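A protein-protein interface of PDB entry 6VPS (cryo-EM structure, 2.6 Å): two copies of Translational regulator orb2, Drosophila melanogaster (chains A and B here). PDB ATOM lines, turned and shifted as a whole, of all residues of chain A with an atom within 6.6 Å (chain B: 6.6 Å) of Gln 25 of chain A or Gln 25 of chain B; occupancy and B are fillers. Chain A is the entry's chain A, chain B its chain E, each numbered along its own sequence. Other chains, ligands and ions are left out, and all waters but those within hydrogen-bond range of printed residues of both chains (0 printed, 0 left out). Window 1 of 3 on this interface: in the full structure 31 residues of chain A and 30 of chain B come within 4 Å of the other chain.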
ATOM      1  N   GLN A   8      11.994 -14.923 -12.186  1.00  0.00           N
ATOM      2  CA  GLN A   8      13.104 -14.796 -11.228  1.00  0.00           C
ATOM      3  C   GLN A   8      14.263 -14.081 -11.911  1.00  0.00           C
ATOM      4  O   GLN A   8      14.714 -14.511 -12.994  1.00  0.00           O
ATOM      5  CB  GLN A   8      13.585 -16.196 -10.776  1.00  0.00           C
ATOM      6  CG  GLN A   8      12.903 -16.726  -9.520  1.00  0.00           C
ATOM      7  CD  GLN A   8      13.082 -18.228  -9.342  1.00  0.00           C
ATOM      8  OE1 GLN A   8      13.553 -18.954 -10.260  1.00  0.00           O
ATOM      9  NE2 GLN A   8      12.697 -18.723  -8.165  1.00  0.00           N
ATOM     10  N   GLN A   9      14.799 -13.042 -11.260  1.00  0.00           N
ATOM     11  CA  GLN A   9      16.023 -12.426 -11.780  1.00  0.00           C
ATOM     12  C   GLN A   9      17.069 -12.252 -10.700  1.00  0.00           C
ATOM     13  O   GLN A   9      16.744 -11.877  -9.555  1.00  0.00           O
ATOM     14  CB  GLN A   9      15.762 -11.188 -12.635  1.00  0.00           C
ATOM     15  CG  GLN A   9      14.886 -10.147 -12.001  1.00  0.00           C
ATOM     16  CD  GLN A   9      14.469  -9.079 -12.986  1.00  0.00           C
ATOM     17  OE1 GLN A   9      15.039  -8.936 -14.072  1.00  0.00           O
ATOM     18  NE2 GLN A   9      13.470  -8.301 -12.604  1.00  0.00           N
ATOM     19  N   GLN A  10      18.313 -12.606 -11.060  1.00  0.00           N
ATOM     20  CA  GLN A  10      19.505 -12.340 -10.241  1.00  0.00           C
ATOM     21  C   GLN A  10      20.477 -11.506 -11.077  1.00  0.00           C
ATOM     22  O   GLN A  10      20.860 -11.929 -12.182  1.00  0.00           O
ATOM     23  CB  GLN A  10      20.166 -13.670  -9.795  1.00  0.00           C
ATOM     24  CG  GLN A  10      19.566 -14.270  -8.509  1.00  0.00           C
ATOM     25  CD  GLN A  10      19.826 -15.762  -8.346  1.00  0.00           C
ATOM     26  OE1 GLN A  10      20.328 -16.440  -9.266  1.00  0.00           O
ATOM     27  NE2 GLN A  10      19.392 -16.316  -7.214  1.00  0.00           N
ATOM     28  N   LEU A  23      24.413 -18.943  -7.069  1.00  0.00           N
ATOM     29  CA  LEU A  23      23.199 -18.323  -7.569  1.00  0.00           C
ATOM     30  C   LEU A  23      22.296 -19.440  -8.065  1.00  0.00           C
ATOM     31  O   LEU A  23      22.589 -20.072  -9.099  1.00  0.00           O
ATOM     32  CB  LEU A  23      23.578 -17.353  -8.696  1.00  0.00           C
ATOM     33  CG  LEU A  23      24.005 -15.955  -8.266  1.00  0.00           C
ATOM     34  CD1 LEU A  23      25.408 -15.960  -7.674  1.00  0.00           C
ATOM     35  CD2 LEU A  23      23.940 -15.005  -9.446  1.00  0.00           C
ATOM     36  N   HIS A  24      21.375 -19.852  -7.207  1.00  0.00           N
ATOM     37  CA  HIS A  24      20.423 -20.907  -7.551  1.00  0.00           C
ATOM     38  C   HIS A  24      19.050 -20.295  -7.748  1.00  0.00           C
ATOM     39  O   HIS A  24      18.653 -19.341  -7.010  1.00  0.00           O
ATOM     40  CB  HIS A  24      20.392 -22.005  -6.475  1.00  0.00           C
ATOM     41  CG  HIS A  24      21.707 -22.674  -6.213  1.00  0.00           C
ATOM     42  ND1 HIS A  24      22.686 -22.827  -7.195  1.00  0.00           N
ATOM     43  CD2 HIS A  24      22.153 -23.362  -5.133  1.00  0.00           C
ATOM     44  CE1 HIS A  24      23.710 -23.487  -6.684  1.00  0.00           C
ATOM     45  NE2 HIS A  24      23.401 -23.841  -5.429  1.00  0.00           N
ATOM     46  N   GLN A  25      18.387 -20.760  -8.792  1.00  0.00           N
ATOM     47  CA  GLN A  25      17.022 -20.358  -9.126  1.00  0.00           C
ATOM     48  C   GLN A  25      16.212 -21.621  -9.371  1.00  0.00           C
ATOM     49  O   GLN A  25      16.555 -22.421 -10.262  1.00  0.00           O
ATOM     50  CB  GLN A  25      17.043 -19.476 -10.399  1.00  0.00           C
ATOM     51  CG  GLN A  25      17.471 -18.046 -10.141  1.00  0.00           C
ATOM     52  CD  GLN A  25      17.530 -17.168 -11.383  1.00  0.00           C
ATOM     53  OE1 GLN A  25      17.925 -17.609 -12.494  1.00  0.00           O
ATOM     54  NE2 GLN A  25      17.253 -15.878 -11.182  1.00  0.00           N
ATOM     55  N   HIS A  26      15.137 -21.787  -8.606  1.00  0.00           N
ATOM     56  CA  HIS A  26      14.231 -22.938  -8.750  1.00  0.00           C
ATOM     57  C   HIS A  26      12.816 -22.437  -9.000  1.00  0.00           C
ATOM     58  O   HIS A  26      12.306 -21.570  -8.237  1.00  0.00           O
ATOM     59  CB  HIS A  26      14.252 -23.797  -7.473  1.00  0.00           C
ATOM     60  CG  HIS A  26      15.548 -24.458  -7.233  1.00  0.00           C
ATOM     61  ND1 HIS A  26      16.563 -23.851  -6.502  1.00  0.00           N
ATOM     62  CD2 HIS A  26      16.050 -25.632  -7.693  1.00  0.00           C
ATOM     63  CE1 HIS A  26      17.624 -24.625  -6.515  1.00  0.00           C
ATOM     64  NE2 HIS A  26      17.341 -25.722  -7.252  1.00  0.00           N
ATOM     65  N   GLN A  27      12.156 -23.043  -9.988  1.00  0.00           N
ATOM     66  CA  GLN A  27      10.761 -22.750 -10.302  1.00  0.00           C
ATOM     67  C   GLN A  27      10.009 -24.049 -10.559  1.00  0.00           C
ATOM     68  O   GLN A  27      10.414 -24.855 -11.419  1.00  0.00           O
ATOM     69  CB  GLN A  27      10.694 -21.891 -11.550  1.00  0.00           C
ATOM     70  CG  GLN A  27      10.800 -20.407 -11.261  1.00  0.00           C
ATOM     71  CD  GLN A  27      10.993 -19.580 -12.517  1.00  0.00           C
ATOM     72  OE1 GLN A  27      11.438 -20.078 -13.583  1.00  0.00           O
ATOM     73  NE2 GLN A  27      10.770 -18.283 -12.371  1.00  0.00           N
ATOM     74  N   HIS B   7      10.108 -17.936 -16.373  1.00  0.00           N
ATOM     75  CA  HIS B   7      11.254 -17.197 -16.855  1.00  0.00           C
ATOM     76  C   HIS B   7      12.275 -17.059 -15.731  1.00  0.00           C
ATOM     77  O   HIS B   7      11.911 -16.791 -14.572  1.00  0.00           O
ATOM     78  CB  HIS B   7      10.803 -15.853 -17.429  1.00  0.00           C
ATOM     79  CG  HIS B   7      11.925 -14.972 -17.853  1.00  0.00           C
ATOM     80  ND1 HIS B   7      12.653 -15.206 -18.998  1.00  0.00           N
ATOM     81  CD2 HIS B   7      12.452 -13.871 -17.288  1.00  0.00           C
ATOM     82  CE1 HIS B   7      13.589 -14.300 -19.109  1.00  0.00           C
ATOM     83  NE2 HIS B   7      13.487 -13.468 -18.074  1.00  0.00           N
ATOM     84  N   GLN B   8      13.554 -17.248 -16.086  1.00  0.00           N
ATOM     85  CA  GLN B   8      14.666 -17.113 -15.146  1.00  0.00           C
ATOM     86  C   GLN B   8      15.793 -16.368 -15.825  1.00  0.00           C
ATOM     87  O   GLN B   8      16.203 -16.740 -16.924  1.00  0.00           O
ATOM     88  CB  GLN B   8      15.176 -18.502 -14.725  1.00  0.00           C
ATOM     89  CG  GLN B   8      14.509 -19.025 -13.471  1.00  0.00           C
ATOM     90  CD  GLN B   8      14.735 -20.503 -13.228  1.00  0.00           C
ATOM     91  OE1 GLN B   8      15.218 -21.248 -14.100  1.00  0.00           O
ATOM     92  NE2 GLN B   8      14.381 -20.946 -12.023  1.00  0.00           N
ATOM     93  N   GLN B   9      16.327 -15.341 -15.156  1.00  0.00           N
ATOM     94  CA  GLN B   9      17.524 -14.696 -15.685  1.00  0.00           C
ATOM     95  C   GLN B   9      18.584 -14.513 -14.623  1.00  0.00           C
ATOM     96  O   GLN B   9      18.272 -14.281 -13.429  1.00  0.00           O
ATOM     97  CB  GLN B   9      17.226 -13.467 -16.532  1.00  0.00           C
ATOM     98  CG  GLN B   9      16.293 -12.477 -15.894  1.00  0.00           C
ATOM     99  CD  GLN B   9      15.837 -11.403 -16.854  1.00  0.00           C
ATOM    100  OE1 GLN B   9      16.275 -11.332 -18.006  1.00  0.00           O
ATOM    101  NE2 GLN B   9      14.950 -10.545 -16.379  1.00  0.00           N
ATOM    102  N   GLN B  10      19.830 -14.749 -15.052  1.00  0.00           N
ATOM    103  CA  GLN B  10      21.032 -14.472 -14.267  1.00  0.00           C
ATOM    104  C   GLN B  10      21.972 -13.637 -15.112  1.00  0.00           C
ATOM    105  O   GLN B  10      22.310 -14.035 -16.227  1.00  0.00           O
ATOM    106  CB  GLN B  10      21.706 -15.782 -13.843  1.00  0.00           C
ATOM    107  CG  GLN B  10      21.081 -16.376 -12.598  1.00  0.00           C
ATOM    108  CD  GLN B  10      21.442 -17.822 -12.334  1.00  0.00           C
ATOM    109  OE1 GLN B  10      21.904 -18.556 -13.209  1.00  0.00           O
ATOM    110  NE2 GLN B  10      21.147 -18.265 -11.133  1.00  0.00           N
ATOM    111  N   LEU B  23      26.080 -21.017 -11.044  1.00  0.00           N
ATOM    112  CA  LEU B  23      24.836 -20.427 -11.504  1.00  0.00           C
ATOM    113  C   LEU B  23      23.951 -21.569 -11.990  1.00  0.00           C
ATOM    114  O   LEU B  23      24.249 -22.186 -13.012  1.00  0.00           O
ATOM    115  CB  LEU B  23      25.157 -19.443 -12.636  1.00  0.00           C
ATOM    116  CG  LEU B  23      25.633 -18.052 -12.227  1.00  0.00           C
ATOM    117  CD1 LEU B  23      27.050 -18.082 -11.664  1.00  0.00           C
ATOM    118  CD2 LEU B  23      25.577 -17.122 -13.415  1.00  0.00           C
ATOM    119  N   HIS B  24      23.041 -22.004 -11.134  1.00  0.00           N
ATOM    120  CA  HIS B  24      22.137 -23.097 -11.479  1.00  0.00           C
ATOM    121  C   HIS B  24      20.743 -22.549 -11.663  1.00  0.00           C
ATOM    122  O   HIS B  24      20.238 -21.812 -10.808  1.00  0.00           O
ATOM    123  CB  HIS B  24      22.125 -24.180 -10.390  1.00  0.00           C
ATOM    124  CG  HIS B  24      23.453 -24.789 -10.089  1.00  0.00           C
ATOM    125  ND1 HIS B  24      24.482 -24.832 -11.014  1.00  0.00           N
ATOM    126  CD2 HIS B  24      23.882 -25.498  -9.016  1.00  0.00           C
ATOM    127  CE1 HIS B  24      25.502 -25.476 -10.495  1.00  0.00           C
ATOM    128  NE2 HIS B  24      25.157 -25.900  -9.270  1.00  0.00           N
ATOM    129  N   GLN B  25      20.097 -23.001 -12.714  1.00  0.00           N
ATOM    130  CA  GLN B  25      18.709 -22.651 -12.983  1.00  0.00           C
ATOM    131  C   GLN B  25      17.927 -23.924 -13.178  1.00  0.00           C
ATOM    132  O   GLN B  25      18.292 -24.736 -14.001  1.00  0.00           O
ATOM    133  CB  GLN B  25      18.661 -21.799 -14.246  1.00  0.00           C
ATOM    134  CG  GLN B  25      19.053 -20.379 -13.971  1.00  0.00           C
ATOM    135  CD  GLN B  25      19.050 -19.501 -15.185  1.00  0.00           C
ATOM    136  OE1 GLN B  25      19.397 -19.932 -16.290  1.00  0.00           O
ATOM    137  NE2 GLN B  25      18.782 -18.215 -14.963  1.00  0.00           N
ATOM    138  N   HIS B  26      16.838 -24.070 -12.441  1.00  0.00           N
ATOM    139  CA  HIS B  26      15.972 -25.242 -12.564  1.00  0.00           C
ATOM    140  C   HIS B  26      14.547 -24.789 -12.797  1.00  0.00           C
ATOM    141  O   HIS B  26      14.025 -23.945 -12.038  1.00  0.00           O
ATOM    142  CB  HIS B  26      16.033 -26.077 -11.291  1.00  0.00           C
ATOM    143  CG  HIS B  26      17.360 -26.653 -11.025  1.00  0.00           C
ATOM    144  ND1 HIS B  26      18.343 -25.954 -10.338  1.00  0.00           N
ATOM    145  CD2 HIS B  26      17.893 -27.854 -11.351  1.00  0.00           C
ATOM    146  CE1 HIS B  26      19.423 -26.689 -10.272  1.00  0.00           C
ATOM    147  NE2 HIS B  26      19.172 -27.865 -10.888  1.00  0.00           N
ATOM    148  N   GLN B  27      13.886 -25.440 -13.744  1.00  0.00           N
ATOM    149  CA  GLN B  27      12.490 -25.171 -14.045  1.00  0.00           C
ATOM    150  C   GLN B  27      11.757 -26.478 -14.280  1.00  0.00           C
ATOM    151  O   GLN B  27      12.223 -27.320 -15.040  1.00  0.00           O
ATOM    152  CB  GLN B  27      12.409 -24.338 -15.298  1.00  0.00           C
ATOM    153  CG  GLN B  27      12.385 -22.860 -14.997  1.00  0.00           C
ATOM    154  CD  GLN B  27      12.527 -22.017 -16.236  1.00  0.00           C
ATOM    155  OE1 GLN B  27      12.940 -22.499 -17.297  1.00  0.00           O
ATOM    156  NE2 GLN B  27      12.353 -20.716 -16.063  1.00  0.00           N
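His 24 of chain B touches its own counterpart, His 24 of chain A.
Gln 25 of chain A touches Gln 10 of chain B, but with the chains exchanged Gln 10 of chain A does not touch Gln 25 of chain B (6.2 Å).
Gln 25 of chain A touches His 24 of chain B, but with the chains exchanged His 24 of chain A does not touch Gln 25 of chain B (5.6 Å).
Gln 25 of chain B touches its own counterpart, Gln 25 of chain A.
8 positions are printed for both chains.
Hydrophobic or aromatic side chains of chain A within 4 Å of the printed part of chain B: Leu 23, His 24 and His 26.
Along chain A the printed residues that touch a printed residue of chain B span positions 8 to 27.
Among the printed residues, no Asp or Glu carboxylate lies within 4 Å of a Lys or Arg side-chain nitrogen of the other chain.
Among the printed residues, pairs that only touch across the chains: His 24 of chain A with His 24 of chain B (3.1 Å), Leu 23 of chain A with Leu 23 of chain B (3.3 Å), Gln 25 of chain A with Gln 10 of chain B (3.4 Å) and His 26 of chain A with Gln 8 of chain B (3.6 Å).
The backbone carbonyl oxygen (O) of His 24 of chain A lies within hydrogen-bond range of the side-chain amide nitrogen (NE2) of Gln 10 of chain A (3.1 Å).
The backbone carbonyl oxygen (O) of Gln 8 of chain A sits at hydrogen-bond distance from the side-chain amide nitrogen (NE2) of Gln 25 of chain A.
O of His 26 of chain B sits at hydrogen-bond distance from NE2 of Gln 8 of chain B.
The backbone NH (N) of Gln 10 of chain A lies close to the side-chain amide nitrogen (NE2) of Gln 25 of chain A (3.4 Å).
NE2 of Gln 8 of chain A is in hydrogen-bond range of O of His 26 of chain A (2.9 Å).
NE2 of Gln 10 of chain B sits at hydrogen-bond distance from O of Leu 23 of chain A, at 3.1 Å.
OE1 of Gln 9 of chain A lies within hydrogen-bond range of NE2 of Gln 9 of chain B (2.8 Å).
OE1 of Gln 25 of chain A sits at hydrogen-bond distance from NE2 of Gln 25 of chain B, at 2.7 Å.
The backbone carbonyl oxygen of His 24 of chain B is in hydrogen-bond range of the backbone NH of Gln 25 of chain A, at 2.9 Å.
N of Gln 9 of chain B sits at hydrogen-bond distance from O of Gln 8 of chain A.
The side-chain amide nitrogen of Gln 8 of chain B lies close to the side-chain amide oxygen of Gln 27 of chain A, 3.4 Å away.
OE1 of Gln 8 of chain A lies within hydrogen-bond range of NE2 of Gln 8 of chain B (2.8 Å).
The side-chain amide oxygen (OE1) of Gln 27 of chain A sits at hydrogen-bond distance from the side-chain amide nitrogen (NE2) of Gln 27 of chain B.
The backbone NH (N) of Gln 10 of chain A lies within hydrogen-bond range of the backbone carbonyl oxygen (O) of Gln 9 of chain B (2.9 Å).
O of Gln 25 of chain A lies within hydrogen-bond range of NE2 of Gln 8 of chain B.
N of Gln 27 of chain A is in hydrogen-bond range of O of His 26 of chain B (2.9 Å).
The backbone NH (N) of Gln 8 of chain A sits at hydrogen-bond distance from the backbone carbonyl oxygen (O) of His 7 of chain B, 3.0 Å away.
A ring nitrogen (NE2) of His 26 of chain A is in hydrogen-bond range of a ring nitrogen (ND1) of His 26 of chain B (3.3 Å).
The backbone carbonyl oxygen (O) of His 7 of chain B is in hydrogen-bond range of the side-chain amide nitrogen (NE2) of Gln 27 of chain A.
N of His 26 of chain B sits at hydrogen-bond distance from O of Gln 25 of chain A (2.7 Å).
OE1 of Gln 10 of chain A lies within hydrogen-bond range of NE2 of Gln 10 of chain B (2.7 Å).
The side-chain amide nitrogen (NE2) of Gln 25 of chain A sits at hydrogen-bond distance from the backbone carbonyl oxygen (O) of Gln 9 of chain B (2.9 Å).
The backbone carbonyl oxygen (O) of Leu 23 of chain A lies within hydrogen-bond range of the backbone NH (N) of His 24 of chain B.
Printed residues of chain B within 4 Å of Gln 10 of chain A: Gln 9 and Gln 10.
Of chain B, only Gln 8 (3.2 Å), Gln 9 (2.9 Å), Gln 10 (3.4 Å), His 24 (2.9 Å), Gln 25 (2.7 Å) and His 26 (2.7 Å) come within 4 Å of Gln 25 of chain A.
Printed residues of chain B within 4 Å of His 26 of chain A: Gln 8 (3.6 Å) and His 26 (3.3 Å).
Printed residues of chain A within 4 Å of Gln 9 of chain B: Gln 8, Gln 9, Gln 10 and Gln 25.
Printed residues of chain A within 4 Å of Leu 23 of chain B: Leu 23.
Of chain A, only Gln 25 comes within 4 Å of Gln 25 of chain B.
The nearest residue of chain B that does not touch Gln 25 of chain A is Gln 27 of chain B (5.3 Å).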
